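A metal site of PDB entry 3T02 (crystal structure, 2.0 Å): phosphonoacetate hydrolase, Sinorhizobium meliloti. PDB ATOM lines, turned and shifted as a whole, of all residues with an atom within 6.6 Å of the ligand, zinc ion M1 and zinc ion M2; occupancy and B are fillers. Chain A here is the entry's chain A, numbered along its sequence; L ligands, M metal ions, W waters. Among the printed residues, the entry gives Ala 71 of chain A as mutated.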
ATOM      1  N   ASP A  32      15.608 -17.912  31.711  1.00  0.00           N
ATOM      2  CA  ASP A  32      14.336 -17.640  31.061  1.00  0.00           C
ATOM      3  C   ASP A  32      14.292 -18.230  29.656  1.00  0.00           C
ATOM      4  O   ASP A  32      15.190 -17.974  28.841  1.00  0.00           O
ATOM      5  CB  ASP A  32      14.132 -16.122  31.008  1.00  0.00           C
ATOM      6  CG  ASP A  32      12.677 -15.737  30.795  1.00  0.00           C
ATOM      7  OD1 ASP A  32      12.003 -16.330  29.931  1.00  0.00           O
ATOM      8  OD2 ASP A  32      12.205 -14.851  31.516  1.00  0.00           O
ATOM      9  N   GLY A  33      13.269 -19.038  29.373  1.00  0.00           N
ATOM     10  CA  GLY A  33      13.038 -19.594  28.034  1.00  0.00           C
ATOM     11  C   GLY A  33      14.040 -20.646  27.591  1.00  0.00           C
ATOM     12  O   GLY A  33      14.166 -20.941  26.390  1.00  0.00           O
ATOM     13  N   SER A  69       2.789 -21.488  30.758  1.00  0.00           N
ATOM     14  CA  SER A  69       4.255 -21.419  30.757  1.00  0.00           C
ATOM     15  C   SER A  69       4.780 -20.025  30.367  1.00  0.00           C
ATOM     16  O   SER A  69       5.400 -19.858  29.325  1.00  0.00           O
ATOM     17  CB  SER A  69       4.886 -22.577  29.948  1.00  0.00           C
ATOM     18  OG  SER A  69       4.347 -22.717  28.636  1.00  0.00           O
ATOM     19  N   PHE A  70       4.507 -19.044  31.242  1.00  0.00           N
ATOM     20  CA  PHE A  70       5.016 -17.676  31.093  1.00  0.00           C
ATOM     21  C   PHE A  70       5.811 -17.279  32.340  1.00  0.00           C
ATOM     22  O   PHE A  70       5.731 -17.942  33.369  1.00  0.00           O
ATOM     23  CB  PHE A  70       3.868 -16.674  30.912  1.00  0.00           C
ATOM     24  CG  PHE A  70       3.054 -16.892  29.657  1.00  0.00           C
ATOM     25  CD1 PHE A  70       3.639 -16.795  28.396  1.00  0.00           C
ATOM     26  CD2 PHE A  70       1.691 -17.164  29.739  1.00  0.00           C
ATOM     27  CE1 PHE A  70       2.875 -16.985  27.227  1.00  0.00           C
ATOM     28  CE2 PHE A  70       0.921 -17.351  28.577  1.00  0.00           C
ATOM     29  CZ  PHE A  70       1.523 -17.256  27.319  1.00  0.00           C
ATOM     30  N   ALA A  71       6.555 -16.176  32.230  1.00  0.00           N
ATOM     31  CA  ALA A  71       7.479 -15.726  33.278  1.00  0.00           C
ATOM     32  C   ALA A  71       6.818 -15.416  34.613  1.00  0.00           C
ATOM     33  O   ALA A  71       7.294 -15.869  35.643  1.00  0.00           O
ATOM     34  CB  ALA A  71       8.272 -14.505  32.790  1.00  0.00           C
ATOM     35  N   ASN A  72       5.745 -14.624  34.616  1.00  0.00           N
ATOM     36  CA  ASN A  72       5.166 -14.189  35.880  1.00  0.00           C
ATOM     37  C   ASN A  72       4.667 -15.332  36.779  1.00  0.00           C
ATOM     38  O   ASN A  72       5.137 -15.434  37.915  1.00  0.00           O
ATOM     39  CB  ASN A  72       4.122 -13.078  35.710  1.00  0.00           C
ATOM     40  CG  ASN A  72       4.762 -11.735  35.492  1.00  0.00           C
ATOM     41  OD1 ASN A  72       5.781 -11.622  34.819  1.00  0.00           O
ATOM     42  ND2 ASN A  72       4.153 -10.685  36.040  1.00  0.00           N
ATOM     43  N   PRO A  73       3.751 -16.199  36.280  1.00  0.00           N
ATOM     44  CA  PRO A  73       3.304 -17.322  37.141  1.00  0.00           C
ATOM     45  C   PRO A  73       4.483 -18.221  37.579  1.00  0.00           C
ATOM     46  O   PRO A  73       4.513 -18.712  38.713  1.00  0.00           O
ATOM     47  CB  PRO A  73       2.382 -18.136  36.233  1.00  0.00           C
ATOM     48  CG  PRO A  73       2.069 -17.268  35.097  1.00  0.00           C
ATOM     49  CD  PRO A  73       3.168 -16.277  34.928  1.00  0.00           C
ATOM     50  N   ASN A  75       8.049 -17.548  37.664  1.00  0.00           N
ATOM     51  CA  ASN A  75       8.987 -16.904  38.602  1.00  0.00           C
ATOM     52  C   ASN A  75       8.392 -16.801  39.997  1.00  0.00           C
ATOM     53  O   ASN A  75       9.080 -17.050  40.997  1.00  0.00           O
ATOM     54  CB  ASN A  75       9.383 -15.508  38.121  1.00  0.00           C
ATOM     55  CG  ASN A  75      10.474 -15.539  37.071  1.00  0.00           C
ATOM     56  OD1 ASN A  75      10.197 -15.540  35.857  1.00  0.00           O
ATOM     57  ND2 ASN A  75      11.712 -15.566  37.528  1.00  0.00           N
ATOM     58  N   ASN A  92       0.047 -11.512  33.400  1.00  0.00           N
ATOM     59  CA  ASN A  92       0.540 -10.133  33.547  1.00  0.00           C
ATOM     60  C   ASN A  92      -0.539  -9.126  33.904  1.00  0.00           C
ATOM     61  O   ASN A  92      -0.246  -8.040  34.408  1.00  0.00           O
ATOM     62  CB  ASN A  92       1.290  -9.679  32.284  1.00  0.00           C
ATOM     63  CG  ASN A  92       2.612 -10.395  32.117  1.00  0.00           C
ATOM     64  OD1 ASN A  92       3.449 -10.406  33.013  1.00  0.00           O
ATOM     65  ND2 ASN A  92       2.811 -10.989  30.946  1.00  0.00           N
ATOM     66  N   LYS A 133      14.538  -7.825  34.291  1.00  0.00           N
ATOM     67  CA  LYS A 133      13.493  -6.810  34.133  1.00  0.00           C
ATOM     68  C   LYS A 133      12.985  -6.296  35.471  1.00  0.00           C
ATOM     69  O   LYS A 133      12.886  -7.063  36.449  1.00  0.00           O
ATOM     70  CB  LYS A 133      12.355  -7.347  33.279  1.00  0.00           C
ATOM     71  CG  LYS A 133      12.632  -7.215  31.775  1.00  0.00           C
ATOM     72  CD  LYS A 133      12.030  -5.944  31.177  1.00  0.00           C
ATOM     73  CE  LYS A 133      10.689  -6.213  30.509  1.00  0.00           C
ATOM     74  NZ  LYS A 133      10.859  -6.792  29.137  1.00  0.00           N
ATOM     75  N   LYS A 135       9.959  -5.151  36.364  1.00  0.00           N
ATOM     76  CA  LYS A 135       8.572  -5.455  36.729  1.00  0.00           C
ATOM     77  C   LYS A 135       8.499  -6.592  37.748  1.00  0.00           C
ATOM     78  O   LYS A 135       7.814  -6.494  38.760  1.00  0.00           O
ATOM     79  CB  LYS A 135       7.713  -5.773  35.490  1.00  0.00           C
ATOM     80  CG  LYS A 135       8.446  -6.479  34.342  1.00  0.00           C
ATOM     81  CD  LYS A 135       8.329  -7.998  34.370  1.00  0.00           C
ATOM     82  CE  LYS A 135       6.881  -8.456  34.125  1.00  0.00           C
ATOM     83  NZ  LYS A 135       6.383  -8.142  32.743  1.00  0.00           N
ATOM     84  N   THR A 212      16.538 -14.175  34.531  1.00  0.00           N
ATOM     85  CA  THR A 212      16.973 -13.481  33.319  1.00  0.00           C
ATOM     86  C   THR A 212      15.776 -13.179  32.427  1.00  0.00           C
ATOM     87  O   THR A 212      14.642 -13.304  32.870  1.00  0.00           O
ATOM     88  CB  THR A 212      17.994 -14.352  32.557  1.00  0.00           C
ATOM     89  OG1 THR A 212      17.436 -15.629  32.290  1.00  0.00           O
ATOM     90  CG2 THR A 212      19.259 -14.533  33.382  1.00  0.00           C
ATOM     91  N   THR A 213      16.007 -12.742  31.175  1.00  0.00           N
ATOM     92  CA  THR A 213      14.881 -12.670  30.216  1.00  0.00           C
ATOM     93  C   THR A 213      15.161 -13.551  29.012  1.00  0.00           C
ATOM     94  O   THR A 213      16.313 -13.974  28.794  1.00  0.00           O
ATOM     95  CB  THR A 213      14.546 -11.234  29.706  1.00  0.00           C
ATOM     96  OG1 THR A 213      15.513 -10.829  28.725  1.00  0.00           O
ATOM     97  CG2 THR A 213      14.468 -10.222  30.836  1.00  0.00           C
ATOM     98  N   ASP A 214      14.125 -13.834  28.233  1.00  0.00           N
ATOM     99  CA  ASP A 214      14.269 -14.721  27.079  1.00  0.00           C
ATOM    100  C   ASP A 214      14.348 -13.990  25.716  1.00  0.00           C
ATOM    101  O   ASP A 214      13.937 -14.534  24.689  1.00  0.00           O
ATOM    102  CB  ASP A 214      13.173 -15.787  27.075  1.00  0.00           C
ATOM    103  CG  ASP A 214      11.768 -15.183  27.032  1.00  0.00           C
ATOM    104  OD1 ASP A 214      11.612 -13.950  27.084  1.00  0.00           O
ATOM    105  OD2 ASP A 214      10.809 -15.967  26.946  1.00  0.00           O
ATOM    106  N   TYR A 215      14.883 -12.773  25.740  1.00  0.00           N
ATOM    107  CA  TYR A 215      15.144 -12.009  24.520  1.00  0.00           C
ATOM    108  C   TYR A 215      15.880 -12.817  23.442  1.00  0.00           C
ATOM    109  O   TYR A 215      15.422 -12.897  22.290  1.00  0.00           O
ATOM    110  CB  TYR A 215      15.916 -10.728  24.840  1.00  0.00           C
ATOM    111  CG  TYR A 215      16.448 -10.049  23.582  1.00  0.00           C
ATOM    112  CD1 TYR A 215      15.612  -9.262  22.786  1.00  0.00           C
ATOM    113  CD2 TYR A 215      17.776 -10.223  23.187  1.00  0.00           C
ATOM    114  CE1 TYR A 215      16.073  -8.659  21.629  1.00  0.00           C
ATOM    115  CE2 TYR A 215      18.250  -9.617  22.026  1.00  0.00           C
ATOM    116  CZ  TYR A 215      17.396  -8.836  21.261  1.00  0.00           C
ATOM    117  OH  TYR A 215      17.877  -8.240  20.115  1.00  0.00           O
ATOM    118  N   HIS A 218      13.695 -16.021  22.151  1.00  0.00           N
ATOM    119  CA  HIS A 218      12.576 -15.675  21.250  1.00  0.00           C
ATOM    120  C   HIS A 218      13.098 -15.396  19.820  1.00  0.00           C
ATOM    121  O   HIS A 218      12.373 -15.591  18.840  1.00  0.00           O
ATOM    122  CB  HIS A 218      11.824 -14.439  21.764  1.00  0.00           C
ATOM    123  CG  HIS A 218      10.704 -14.744  22.709  1.00  0.00           C
ATOM    124  ND1 HIS A 218       9.548 -15.366  22.307  1.00  0.00           N
ATOM    125  CD2 HIS A 218      10.531 -14.455  24.023  1.00  0.00           C
ATOM    126  CE1 HIS A 218       8.724 -15.476  23.334  1.00  0.00           C
ATOM    127  NE2 HIS A 218       9.296 -14.929  24.388  1.00  0.00           N
ATOM    128  N   ASP A 253      11.857 -20.793  33.693  1.00  0.00           N
ATOM    129  CA  ASP A 253      10.438 -20.529  33.853  1.00  0.00           C
ATOM    130  C   ASP A 253       9.543 -21.265  32.827  1.00  0.00           C
ATOM    131  O   ASP A 253       8.364 -21.519  33.096  1.00  0.00           O
ATOM    132  CB  ASP A 253      10.172 -19.011  33.845  1.00  0.00           C
ATOM    133  CG  ASP A 253      10.585 -18.323  32.534  1.00  0.00           C
ATOM    134  OD1 ASP A 253      11.351 -18.880  31.712  1.00  0.00           O
ATOM    135  OD2 ASP A 253      10.134 -17.188  32.347  1.00  0.00           O
ATOM    136  N   HIS A 254      10.120 -21.611  31.681  1.00  0.00           N
ATOM    137  CA  HIS A 254       9.423 -22.276  30.566  1.00  0.00           C
ATOM    138  C   HIS A 254      10.445 -22.530  29.472  1.00  0.00           C
ATOM    139  O   HIS A 254      11.542 -21.983  29.506  1.00  0.00           O
ATOM    140  CB  HIS A 254       8.286 -21.397  30.026  1.00  0.00           C
ATOM    141  CG  HIS A 254       8.742 -20.031  29.612  1.00  0.00           C
ATOM    142  ND1 HIS A 254       9.436 -19.798  28.446  1.00  0.00           N
ATOM    143  CD2 HIS A 254       8.628 -18.831  30.229  1.00  0.00           C
ATOM    144  CE1 HIS A 254       9.727 -18.518  28.359  1.00  0.00           C
ATOM    145  NE2 HIS A 254       9.261 -17.909  29.424  1.00  0.00           N
ATOM    146  N   GLY A 255      10.092 -23.384  28.513  1.00  0.00           N
ATOM    147  CA  GLY A 255      10.937 -23.621  27.363  1.00  0.00           C
ATOM    148  C   GLY A 255      10.528 -22.712  26.225  1.00  0.00           C
ATOM    149  O   GLY A 255       9.979 -21.620  26.442  1.00  0.00           O
ATOM    150  N   MET A 256      10.789 -23.168  25.001  1.00  0.00           N
ATOM    151  CA  MET A 256      10.655 -22.308  23.823  1.00  0.00           C
ATOM    152  C   MET A 256      10.556 -23.181  22.590  1.00  0.00           C
ATOM    153  O   MET A 256      11.329 -24.119  22.436  1.00  0.00           O
ATOM    154  CB  MET A 256      11.883 -21.388  23.710  1.00  0.00           C
ATOM    155  CG  MET A 256      11.762 -20.268  22.670  1.00  0.00           C
ATOM    156  SD  MET A 256      10.503 -19.041  23.076  1.00  0.00           S
ATOM    157  CE  MET A 256      11.384 -18.029  24.264  1.00  0.00           C
ATOM    158  N   ILE A 290       0.283 -13.299  28.327  1.00  0.00           N
ATOM    159  CA  ILE A 290       1.692 -13.021  27.986  1.00  0.00           C
ATOM    160  C   ILE A 290       2.036 -11.530  27.996  1.00  0.00           C
ATOM    161  O   ILE A 290       3.171 -11.152  28.275  1.00  0.00           O
ATOM    162  CB  ILE A 290       2.105 -13.647  26.617  1.00  0.00           C
ATOM    163  CG1 ILE A 290       3.615 -13.509  26.378  1.00  0.00           C
ATOM    164  CG2 ILE A 290       1.288 -13.053  25.449  1.00  0.00           C
ATOM    165  CD1 ILE A 290       4.188 -14.350  25.240  1.00  0.00           C
ATOM    166  N   GLY A 299       5.460  -9.652  20.522  1.00  0.00           N
ATOM    167  CA  GLY A 299       5.791 -10.184  21.847  1.00  0.00           C
ATOM    168  C   GLY A 299       4.517 -10.403  22.665  1.00  0.00           C
ATOM    169  O   GLY A 299       4.570 -10.600  23.877  1.00  0.00           O
ATOM    170  N   ARG A 378       8.970 -17.435  17.643  1.00  0.00           N
ATOM    171  CA  ARG A 378       9.265 -18.461  18.635  1.00  0.00           C
ATOM    172  C   ARG A 378       8.566 -18.028  19.931  1.00  0.00           C
ATOM    173  O   ARG A 378       8.653 -16.869  20.326  1.00  0.00           O
ATOM    174  CB  ARG A 378      10.763 -18.580  18.869  1.00  0.00           C
ATOM    175  CG  ARG A 378      11.586 -18.949  17.635  1.00  0.00           C
ATOM    176  CD  ARG A 378      13.100 -18.966  17.934  1.00  0.00           C
ATOM    177  NE  ARG A 378      13.450 -19.824  19.071  1.00  0.00           N
ATOM    178  CZ  ARG A 378      13.376 -21.159  19.075  1.00  0.00           C
ATOM    179  NH1 ARG A 378      12.933 -21.810  18.001  1.00  0.00           N
ATOM    180  NH2 ARG A 378      13.715 -21.833  20.163  1.00  0.00           N
ATOM    181  N   SER A 379       7.883 -18.962  20.594  1.00  0.00           N
ATOM    182  CA  SER A 379       7.171 -18.618  21.820  1.00  0.00           C
ATOM    183  C   SER A 379       6.881 -19.788  22.754  1.00  0.00           C
ATOM    184  O   SER A 379       7.435 -20.887  22.596  1.00  0.00           O
ATOM    185  CB  SER A 379       5.878 -17.854  21.490  1.00  0.00           C
ATOM    186  OG  SER A 379       5.584 -16.926  22.522  1.00  0.00           O
ATOM    187  N   HIS A 380       5.967 -19.541  23.695  1.00  0.00           N
ATOM    188  CA  HIS A 380       5.687 -20.449  24.810  1.00  0.00           C
ATOM    189  C   HIS A 380       4.298 -20.156  25.400  1.00  0.00           C
ATOM    190  O   HIS A 380       3.527 -19.346  24.851  1.00  0.00           O
ATOM    191  CB  HIS A 380       6.782 -20.326  25.883  1.00  0.00           C
ATOM    192  CG  HIS A 380       7.111 -18.901  26.224  1.00  0.00           C
ATOM    193  ND1 HIS A 380       6.597 -18.264  27.333  1.00  0.00           N
ATOM    194  CD2 HIS A 380       7.869 -17.986  25.590  1.00  0.00           C
ATOM    195  CE1 HIS A 380       7.031 -17.020  27.374  1.00  0.00           C
ATOM    196  NE2 HIS A 380       7.823 -16.822  26.321  1.00  0.00           N
HETATM  197  P1  LIG L   1       7.991 -14.033  29.422  1.00  0.00           P
HETATM  198  O1  LIG L   1       6.817 -14.861  29.903  1.00  0.00           O
HETATM  199  O2  LIG L   1       9.341 -14.692  29.586  1.00  0.00           O
HETATM  200  O3  LIG L   1       7.987 -12.611  29.968  1.00  0.00           O
HETATM  201  C1  LIG L   1       7.691 -13.848  27.662  1.00  0.00           C
HETATM  202  C2  LIG L   1       8.310 -12.575  27.179  1.00  0.00           C
HETATM  203  O4  LIG L   1       7.726 -11.499  27.416  1.00  0.00           O
HETATM  204  O5  LIG L   1       9.388 -12.658  26.550  1.00  0.00           O
HETATM  205 ZN    ZN M   1       8.999 -15.164  26.466  1.00  0.00          ZN
HETATM  206 ZN    ZN M   2      10.098 -16.410  30.252  1.00  0.00          ZN
HETATM  207  O   HOH W   1       6.004 -10.168  28.764  1.00  0.00           O
HETATM  208  O   HOH W   2       7.231 -10.911  32.140  1.00  0.00           O
HETATM  209  O   HOH W   3      11.358 -12.613  29.937  1.00  0.00           O
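N of Ala 71 lies within hydrogen-bond range of O1 of the ligand.
ND1 of His 254 lies close to ND1 of His 380, at 3.4 Å.
O of His 254 sits close to N of Gly 33 (3.4 Å).
OG1 of Thr 212 lies within hydrogen-bond range of N of Asp 32 (3.0 Å).
A ring nitrogen (ND1) of His 380 is in hydrogen-bond range of the backbone carbonyl oxygen of Ser 69, 2.8 Å away.
A ring nitrogen (ND1) of His 218 lies within hydrogen-bond range of the backbone carbonyl oxygen (O) of Arg 378.
The side-chain carboxylate of Asp 253 lies within hydrogen-bond range of the backbone NH of Gly 33 (3.0 Å).
The backbone carbonyl oxygen (O) of Ala 71 lies close to the side-chain amide oxygen (OD1) of Asn 75 (2.9 Å).
Merely in contact with the ligand: Phe 70.
Hydrophobic or aromatic side chains within 4 Å of the ligand: Phe 70, Ala 71, His 218 and His 380.
Of the 25 residues printed, 8 come within 4 Å of the ligand.
The nearest printed residue that does not touch the ligand is Ile 290 (4.3 Å).
Within 4 Å of zinc ion M1: Asp 214, His 218, His 254 and His 380.
The nearest printed residue that does not touch zinc ion M1 is Met 256 (4.3 Å).
Residues that only touch zinc ion M2: Ala 71 (3.7 Å).
The nearest printed residue that does not touch zinc ion M2 is Gly 33 (4.2 Å).
Zinc ion M1 is bound by OD2 of Asp 214, 2.0 Å away.
A ring nitrogen (NE2) of His 380 binds zinc ion M1, at 2.0 Å.
NE2 of His 218 is bound to zinc ion M1 (2.1 Å).
Zinc ion M1 is bound by O5 of the ligand (2.5 Å).
NE2 of His 254 binds zinc ion M2 (1.9 Å).
The side-chain carboxylate (OD1) of Asp 32 binds zinc ion M2, at 1.9 Å.
Zinc ion M2 is bound by O2 of the ligand (2.0 Å).
OD2 of Asp 253 binds zinc ion M2 (2.2 Å).
Water W1 bridges an oxygen (O4) of the ligand and the backbone carbonyl oxygen (O) of Ile 290.
Water W2 lies within hydrogen-bond range of an oxygen (O3) of the ligand (2.9 Å), the side-chain amino group of Lys 135 (3.0 Å) and the side-chain amide oxygen of Asn 72 (3.1 Å).
Water W3 lies within hydrogen-bond range of the side-chain carboxylate (OD2) of Asp 32, the side-chain carboxylate (OD1) of Asp 214 and an oxygen (O3) of the ligand.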
